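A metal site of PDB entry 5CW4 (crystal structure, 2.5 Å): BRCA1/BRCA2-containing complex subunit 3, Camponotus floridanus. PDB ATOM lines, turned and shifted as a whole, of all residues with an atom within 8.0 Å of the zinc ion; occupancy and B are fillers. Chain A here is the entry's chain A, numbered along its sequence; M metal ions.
Ser 106 touches the zinc ion. Of the 24 residues printed, 4 come within 4 Å of the zinc ion.
N of Asp 109 lies close to OG of Ser 106, at 3.3 Å. The backbone carbonyl oxygen (O) of Thr 102 is in hydrogen-bond range of a ring nitrogen (ND1) of His 98. O of Leu 126 lies within hydrogen-bond range of N of His 96 (3.1 Å). OD1 of Asp 62 lies within hydrogen-bond range of OG of Ser 106 (2.9 Å).
The zinc ion is bound by OD2 of Asp 109 (2.0 Å), NE2 of His 98 (2.3 Å), NE2 of His 96 (2.4 Å) and OD1 of Asp 109 (2.6 Å). The zinc ion has four donor atoms within binding distance.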
ATOM      1  N   GLU A  32     -19.385 -20.027 -20.494  1.00  0.00           N
ATOM      2  CA  GLU A  32     -19.461 -21.419 -20.905  1.00  0.00           C
ATOM      3  C   GLU A  32     -20.465 -22.155 -20.035  1.00  0.00           C
ATOM      4  O   GLU A  32     -20.584 -21.873 -18.845  1.00  0.00           O
ATOM      5  CB  GLU A  32     -18.093 -22.077 -20.817  1.00  0.00           C
ATOM      6  CG  GLU A  32     -17.081 -21.479 -21.771  1.00  0.00           C
ATOM      7  CD  GLU A  32     -15.660 -21.617 -21.287  1.00  0.00           C
ATOM      8  OE1 GLU A  32     -15.466 -21.692 -20.048  1.00  0.00           O
ATOM      9  OE2 GLU A  32     -14.749 -21.652 -22.134  1.00  0.00           O
ATOM     10  N   VAL A  33     -21.201 -23.074 -20.647  1.00  0.00           N
ATOM     11  CA  VAL A  33     -22.134 -23.906 -19.897  1.00  0.00           C
ATOM     12  C   VAL A  33     -21.659 -25.355 -19.967  1.00  0.00           C
ATOM     13  O   VAL A  33     -20.804 -25.696 -20.778  1.00  0.00           O
ATOM     14  CB  VAL A  33     -23.567 -23.786 -20.437  1.00  0.00           C
ATOM     15  CG1 VAL A  33     -24.004 -22.327 -20.412  1.00  0.00           C
ATOM     16  CG2 VAL A  33     -23.661 -24.349 -21.844  1.00  0.00           C
ATOM     17  N   LYS A  61     -12.926 -18.080 -17.311  1.00  0.00           N
ATOM     18  CA  LYS A  61     -13.049 -18.223 -18.754  1.00  0.00           C
ATOM     19  C   LYS A  61     -12.680 -19.605 -19.281  1.00  0.00           C
ATOM     20  O   LYS A  61     -13.208 -20.055 -20.296  1.00  0.00           O
ATOM     21  CB  LYS A  61     -12.206 -17.172 -19.462  1.00  0.00           C
ATOM     22  N   ASP A  62     -11.760 -20.289 -18.607  1.00  0.00           N
ATOM     23  CA  ASP A  62     -11.320 -21.605 -19.062  1.00  0.00           C
ATOM     24  C   ASP A  62     -11.511 -22.665 -17.962  1.00  0.00           C
ATOM     25  O   ASP A  62     -11.312 -23.850 -18.198  1.00  0.00           O
ATOM     26  CB  ASP A  62      -9.856 -21.567 -19.506  1.00  0.00           C
ATOM     27  CG  ASP A  62      -9.530 -22.612 -20.564  1.00  0.00           C
ATOM     28  OD1 ASP A  62     -10.364 -23.515 -20.787  1.00  0.00           O
ATOM     29  OD2 ASP A  62      -8.444 -22.529 -21.178  1.00  0.00           O
ATOM     30  N   ARG A  63     -11.891 -22.213 -16.779  1.00  0.00           N
ATOM     31  CA  ARG A  63     -12.041 -23.100 -15.630  1.00  0.00           C
ATOM     32  C   ARG A  63     -13.436 -23.728 -15.585  1.00  0.00           C
ATOM     33  O   ARG A  63     -14.319 -23.236 -14.882  1.00  0.00           O
ATOM     34  CB  ARG A  63     -11.771 -22.347 -14.325  1.00  0.00           C
ATOM     35  CG  ARG A  63     -10.899 -23.107 -13.336  1.00  0.00           C
ATOM     36  CD  ARG A  63     -11.382 -22.885 -11.919  1.00  0.00           C
ATOM     37  NE  ARG A  63     -11.691 -21.490 -11.651  1.00  0.00           N
ATOM     38  CZ  ARG A  63     -10.949 -20.688 -10.903  1.00  0.00           C
ATOM     39  NH1 ARG A  63      -9.841 -21.144 -10.326  1.00  0.00           N
ATOM     40  NH2 ARG A  63     -11.308 -19.426 -10.718  1.00  0.00           N
ATOM     41  N   VAL A  64     -13.622 -24.799 -16.340  1.00  0.00           N
ATOM     42  CA  VAL A  64     -14.914 -25.488 -16.395  1.00  0.00           C
ATOM     43  C   VAL A  64     -14.818 -26.865 -15.738  1.00  0.00           C
ATOM     44  O   VAL A  64     -14.422 -27.840 -16.367  1.00  0.00           O
ATOM     45  CB  VAL A  64     -15.396 -25.641 -17.864  1.00  0.00           C
ATOM     46  CG1 VAL A  64     -16.630 -26.507 -17.935  1.00  0.00           C
ATOM     47  CG2 VAL A  64     -15.681 -24.269 -18.475  1.00  0.00           C
ATOM     48  N   TRP A  94     -19.239 -35.932 -20.852  1.00  0.00           N
ATOM     49  CA  TRP A  94     -19.614 -34.567 -20.515  1.00  0.00           C
ATOM     50  C   TRP A  94     -19.612 -33.667 -21.747  1.00  0.00           C
ATOM     51  O   TRP A  94     -19.137 -34.061 -22.810  1.00  0.00           O
ATOM     52  CB  TRP A  94     -18.678 -34.002 -19.443  1.00  0.00           C
ATOM     53  CG  TRP A  94     -17.286 -33.749 -19.915  1.00  0.00           C
ATOM     54  CD1 TRP A  94     -16.431 -34.642 -20.501  1.00  0.00           C
ATOM     55  CD2 TRP A  94     -16.574 -32.502 -19.835  1.00  0.00           C
ATOM     56  NE1 TRP A  94     -15.236 -34.028 -20.795  1.00  0.00           N
ATOM     57  CE2 TRP A  94     -15.295 -32.718 -20.393  1.00  0.00           C
ATOM     58  CE3 TRP A  94     -16.896 -31.233 -19.355  1.00  0.00           C
ATOM     59  CZ2 TRP A  94     -14.335 -31.707 -20.486  1.00  0.00           C
ATOM     60  CZ3 TRP A  94     -15.946 -30.233 -19.438  1.00  0.00           C
ATOM     61  CH2 TRP A  94     -14.679 -30.474 -20.006  1.00  0.00           C
ATOM     62  N   HIS A  96     -19.555 -29.169 -22.924  1.00  0.00           N
ATOM     63  CA  HIS A  96     -19.609 -27.762 -22.564  1.00  0.00           C
ATOM     64  C   HIS A  96     -19.510 -26.913 -23.826  1.00  0.00           C
ATOM     65  O   HIS A  96     -19.247 -27.426 -24.914  1.00  0.00           O
ATOM     66  CB  HIS A  96     -18.518 -27.393 -21.556  1.00  0.00           C
ATOM     67  CG  HIS A  96     -17.126 -27.460 -22.095  1.00  0.00           C
ATOM     68  ND1 HIS A  96     -16.642 -28.554 -22.778  1.00  0.00           N
ATOM     69  CD2 HIS A  96     -16.104 -26.578 -22.030  1.00  0.00           C
ATOM     70  CE1 HIS A  96     -15.382 -28.343 -23.127  1.00  0.00           C
ATOM     71  NE2 HIS A  96     -15.037 -27.149 -22.680  1.00  0.00           N
ATOM     72  N   SER A  97     -19.716 -25.611 -23.665  1.00  0.00           N
ATOM     73  CA  SER A  97     -19.855 -24.726 -24.802  1.00  0.00           C
ATOM     74  C   SER A  97     -18.684 -23.776 -24.951  1.00  0.00           C
ATOM     75  O   SER A  97     -18.057 -23.376 -23.966  1.00  0.00           O
ATOM     76  CB  SER A  97     -21.157 -23.925 -24.673  1.00  0.00           C
ATOM     77  OG  SER A  97     -21.167 -23.184 -23.463  1.00  0.00           O
ATOM     78  N   HIS A  98     -18.378 -23.416 -26.201  1.00  0.00           N
ATOM     79  CA  HIS A  98     -17.387 -22.400 -26.498  1.00  0.00           C
ATOM     80  C   HIS A  98     -18.058 -21.210 -27.178  1.00  0.00           C
ATOM     81  O   HIS A  98     -18.138 -21.159 -28.412  1.00  0.00           O
ATOM     82  CB  HIS A  98     -16.286 -22.951 -27.393  1.00  0.00           C
ATOM     83  CG  HIS A  98     -15.294 -23.811 -26.667  1.00  0.00           C
ATOM     84  ND1 HIS A  98     -14.177 -24.333 -27.295  1.00  0.00           N
ATOM     85  CD2 HIS A  98     -15.237 -24.236 -25.387  1.00  0.00           C
ATOM     86  CE1 HIS A  98     -13.482 -25.044 -26.415  1.00  0.00           C
ATOM     87  NE2 HIS A  98     -14.112 -25.002 -25.256  1.00  0.00           N
ATOM     88  N   PRO A  99     -18.554 -20.248 -26.384  1.00  0.00           N
ATOM     89  CA  PRO A  99     -19.110 -19.036 -26.997  1.00  0.00           C
ATOM     90  C   PRO A  99     -17.999 -18.131 -27.528  1.00  0.00           C
ATOM     91  O   PRO A  99     -17.067 -17.807 -26.804  1.00  0.00           O
ATOM     92  CB  PRO A  99     -19.871 -18.379 -25.841  1.00  0.00           C
ATOM     93  CG  PRO A  99     -19.230 -18.907 -24.601  1.00  0.00           C
ATOM     94  CD  PRO A  99     -18.763 -20.299 -24.928  1.00  0.00           C
ATOM     95  N   ILE A 101     -15.557 -18.595 -29.560  1.00  0.00           N
ATOM     96  CA  ILE A 101     -14.240 -19.179 -29.775  1.00  0.00           C
ATOM     97  C   ILE A 101     -14.354 -20.477 -30.556  1.00  0.00           C
ATOM     98  O   ILE A 101     -15.462 -20.974 -30.764  1.00  0.00           O
ATOM     99  CB  ILE A 101     -13.511 -19.454 -28.445  1.00  0.00           C
ATOM    100  CG1 ILE A 101     -14.330 -20.435 -27.582  1.00  0.00           C
ATOM    101  CG2 ILE A 101     -13.239 -18.164 -27.692  1.00  0.00           C
ATOM    102  CD1 ILE A 101     -13.693 -20.747 -26.250  1.00  0.00           C
ATOM    103  N   THR A 102     -13.220 -21.009 -31.000  1.00  0.00           N
ATOM    104  CA  THR A 102     -13.212 -22.244 -31.767  1.00  0.00           C
ATOM    105  C   THR A 102     -13.659 -23.440 -30.929  1.00  0.00           C
ATOM    106  O   THR A 102     -13.594 -23.409 -29.701  1.00  0.00           O
ATOM    107  CB  THR A 102     -11.824 -22.550 -32.358  1.00  0.00           C
ATOM    108  OG1 THR A 102     -10.859 -22.621 -31.305  1.00  0.00           O
ATOM    109  CG2 THR A 102     -11.412 -21.461 -33.331  1.00  0.00           C
ATOM    110  N   VAL A 103     -14.116 -24.484 -31.612  1.00  0.00           N
ATOM    111  CA  VAL A 103     -14.626 -25.673 -30.954  1.00  0.00           C
ATOM    112  C   VAL A 103     -13.488 -26.530 -30.393  1.00  0.00           C
ATOM    113  O   VAL A 103     -13.694 -27.376 -29.516  1.00  0.00           O
ATOM    114  CB  VAL A 103     -15.478 -26.510 -31.926  1.00  0.00           C
ATOM    115  CG1 VAL A 103     -14.600 -27.073 -33.047  1.00  0.00           C
ATOM    116  CG2 VAL A 103     -16.220 -27.616 -31.178  1.00  0.00           C
ATOM    117  N   CYS A 104     -12.277 -26.299 -30.882  1.00  0.00           N
ATOM    118  CA  CYS A 104     -11.105 -27.065 -30.476  1.00  0.00           C
ATOM    119  C   CYS A 104     -10.898 -27.003 -28.966  1.00  0.00           C
ATOM    120  O   CYS A 104     -10.808 -25.921 -28.389  1.00  0.00           O
ATOM    121  CB  CYS A 104      -9.848 -26.566 -31.191  1.00  0.00           C
ATOM    122  SG  CYS A 104      -9.951 -26.601 -32.994  1.00  0.00           S
ATOM    123  N   PRO A 105     -10.831 -28.189 -28.333  1.00  0.00           N
ATOM    124  CA  PRO A 105     -10.569 -28.363 -26.899  1.00  0.00           C
ATOM    125  C   PRO A 105      -9.325 -27.609 -26.432  1.00  0.00           C
ATOM    126  O   PRO A 105      -8.262 -27.729 -27.047  1.00  0.00           O
ATOM    127  CB  PRO A 105     -10.357 -29.876 -26.770  1.00  0.00           C
ATOM    128  CG  PRO A 105     -11.163 -30.457 -27.878  1.00  0.00           C
ATOM    129  CD  PRO A 105     -11.059 -29.470 -29.012  1.00  0.00           C
ATOM    130  N   SER A 106      -9.474 -26.839 -25.359  1.00  0.00           N
ATOM    131  CA  SER A 106      -8.353 -26.084 -24.796  1.00  0.00           C
ATOM    132  C   SER A 106      -7.443 -27.000 -23.974  1.00  0.00           C
ATOM    133  O   SER A 106      -7.759 -28.173 -23.785  1.00  0.00           O
ATOM    134  CB  SER A 106      -8.863 -24.943 -23.928  1.00  0.00           C
ATOM    135  OG  SER A 106      -9.650 -25.421 -22.844  1.00  0.00           O
ATOM    136  N   HIS A 107      -6.325 -26.464 -23.515  1.00  0.00           N
ATOM    137  CA  HIS A 107      -5.398 -27.226 -22.682  1.00  0.00           C
ATOM    138  C   HIS A 107      -6.112 -27.758 -21.437  1.00  0.00           C
ATOM    139  O   HIS A 107      -5.924 -28.903 -21.034  1.00  0.00           O
ATOM    140  CB  HIS A 107      -4.202 -26.367 -22.270  1.00  0.00           C
ATOM    141  CG  HIS A 107      -3.373 -25.895 -23.424  1.00  0.00           C
ATOM    142  ND1 HIS A 107      -2.388 -26.657 -23.995  1.00  0.00           N
ATOM    143  CD2 HIS A 107      -3.391 -24.725 -24.109  1.00  0.00           C
ATOM    144  CE1 HIS A 107      -1.828 -25.991 -24.991  1.00  0.00           C
ATOM    145  NE2 HIS A 107      -2.419 -24.815 -25.074  1.00  0.00           N
ATOM    146  N   VAL A 108      -6.938 -26.909 -20.839  1.00  0.00           N
ATOM    147  CA  VAL A 108      -7.723 -27.303 -19.668  1.00  0.00           C
ATOM    148  C   VAL A 108      -8.746 -28.373 -20.039  1.00  0.00           C
ATOM    149  O   VAL A 108      -9.005 -29.297 -19.260  1.00  0.00           O
ATOM    150  CB  VAL A 108      -8.434 -26.093 -19.049  1.00  0.00           C
ATOM    151  CG1 VAL A 108      -9.483 -26.549 -18.046  1.00  0.00           C
ATOM    152  CG2 VAL A 108      -7.417 -25.163 -18.404  1.00  0.00           C
ATOM    153  N   ASP A 109      -9.328 -28.263 -21.229  1.00  0.00           N
ATOM    154  CA  ASP A 109     -10.313 -29.234 -21.691  1.00  0.00           C
ATOM    155  C   ASP A 109      -9.699 -30.619 -21.862  1.00  0.00           C
ATOM    156  O   ASP A 109     -10.302 -31.625 -21.488  1.00  0.00           O
ATOM    157  CB  ASP A 109     -10.943 -28.785 -23.017  1.00  0.00           C
ATOM    158  CG  ASP A 109     -11.889 -27.626 -22.839  1.00  0.00           C
ATOM    159  OD1 ASP A 109     -12.281 -27.358 -21.687  1.00  0.00           O
ATOM    160  OD2 ASP A 109     -12.249 -26.996 -23.858  1.00  0.00           O
ATOM    161  N   VAL A 110      -8.503 -30.664 -22.446  1.00  0.00           N
ATOM    162  CA  VAL A 110      -7.804 -31.932 -22.630  1.00  0.00           C
ATOM    163  C   VAL A 110      -7.413 -32.538 -21.291  1.00  0.00           C
ATOM    164  O   VAL A 110      -7.557 -33.738 -21.075  1.00  0.00           O
ATOM    165  CB  VAL A 110      -6.557 -31.783 -23.500  1.00  0.00           C
ATOM    166  CG1 VAL A 110      -5.770 -33.086 -23.530  1.00  0.00           C
ATOM    167  CG2 VAL A 110      -6.929 -31.335 -24.914  1.00  0.00           C
ATOM    168  N   LEU A 126     -17.754 -33.791 -25.432  1.00  0.00           N
ATOM    169  CA  LEU A 126     -18.406 -33.011 -26.483  1.00  0.00           C
ATOM    170  C   LEU A 126     -18.268 -31.509 -26.251  1.00  0.00           C
ATOM    171  O   LEU A 126     -18.552 -31.012 -25.152  1.00  0.00           O
ATOM    172  CB  LEU A 126     -19.889 -33.370 -26.588  1.00  0.00           C
ATOM    173  CG  LEU A 126     -20.286 -34.754 -27.091  1.00  0.00           C
ATOM    174  CD1 LEU A 126     -21.801 -34.897 -27.068  1.00  0.00           C
ATOM    175  CD2 LEU A 126     -19.748 -34.988 -28.487  1.00  0.00           C
ATOM    176  N   ILE A 127     -17.850 -30.782 -27.280  1.00  0.00           N
ATOM    177  CA  ILE A 127     -17.791 -29.331 -27.207  1.00  0.00           C
ATOM    178  C   ILE A 127     -18.689 -28.698 -28.261  1.00  0.00           C
ATOM    179  O   ILE A 127     -18.598 -29.038 -29.450  1.00  0.00           O
ATOM    180  CB  ILE A 127     -16.358 -28.814 -27.380  1.00  0.00           C
ATOM    181  CG1 ILE A 127     -15.473 -29.330 -26.240  1.00  0.00           C
ATOM    182  CG2 ILE A 127     -16.335 -27.292 -27.410  1.00  0.00           C
ATOM    183  CD1 ILE A 127     -14.037 -28.868 -26.338  1.00  0.00           C
ATOM    184  N   PHE A 147     -14.472 -35.609 -28.731  1.00  0.00           N
ATOM    185  CA  PHE A 147     -13.046 -35.856 -28.521  1.00  0.00           C
ATOM    186  C   PHE A 147     -12.716 -36.651 -27.258  1.00  0.00           C
ATOM    187  O   PHE A 147     -13.513 -36.689 -26.314  1.00  0.00           O
ATOM    188  CB  PHE A 147     -12.295 -34.528 -28.456  1.00  0.00           C
ATOM    189  CG  PHE A 147     -12.452 -33.816 -27.133  1.00  0.00           C
ATOM    190  CD1 PHE A 147     -13.649 -33.194 -26.808  1.00  0.00           C
ATOM    191  CD2 PHE A 147     -11.417 -33.786 -26.218  1.00  0.00           C
ATOM    192  CE1 PHE A 147     -13.803 -32.532 -25.601  1.00  0.00           C
ATOM    193  CE2 PHE A 147     -11.556 -33.137 -25.000  1.00  0.00           C
ATOM    194  CZ  PHE A 147     -12.750 -32.508 -24.696  1.00  0.00           C
HETATM  195 ZN    ZN M   1     -13.331 -25.461 -23.100  1.00  0.00          ZN
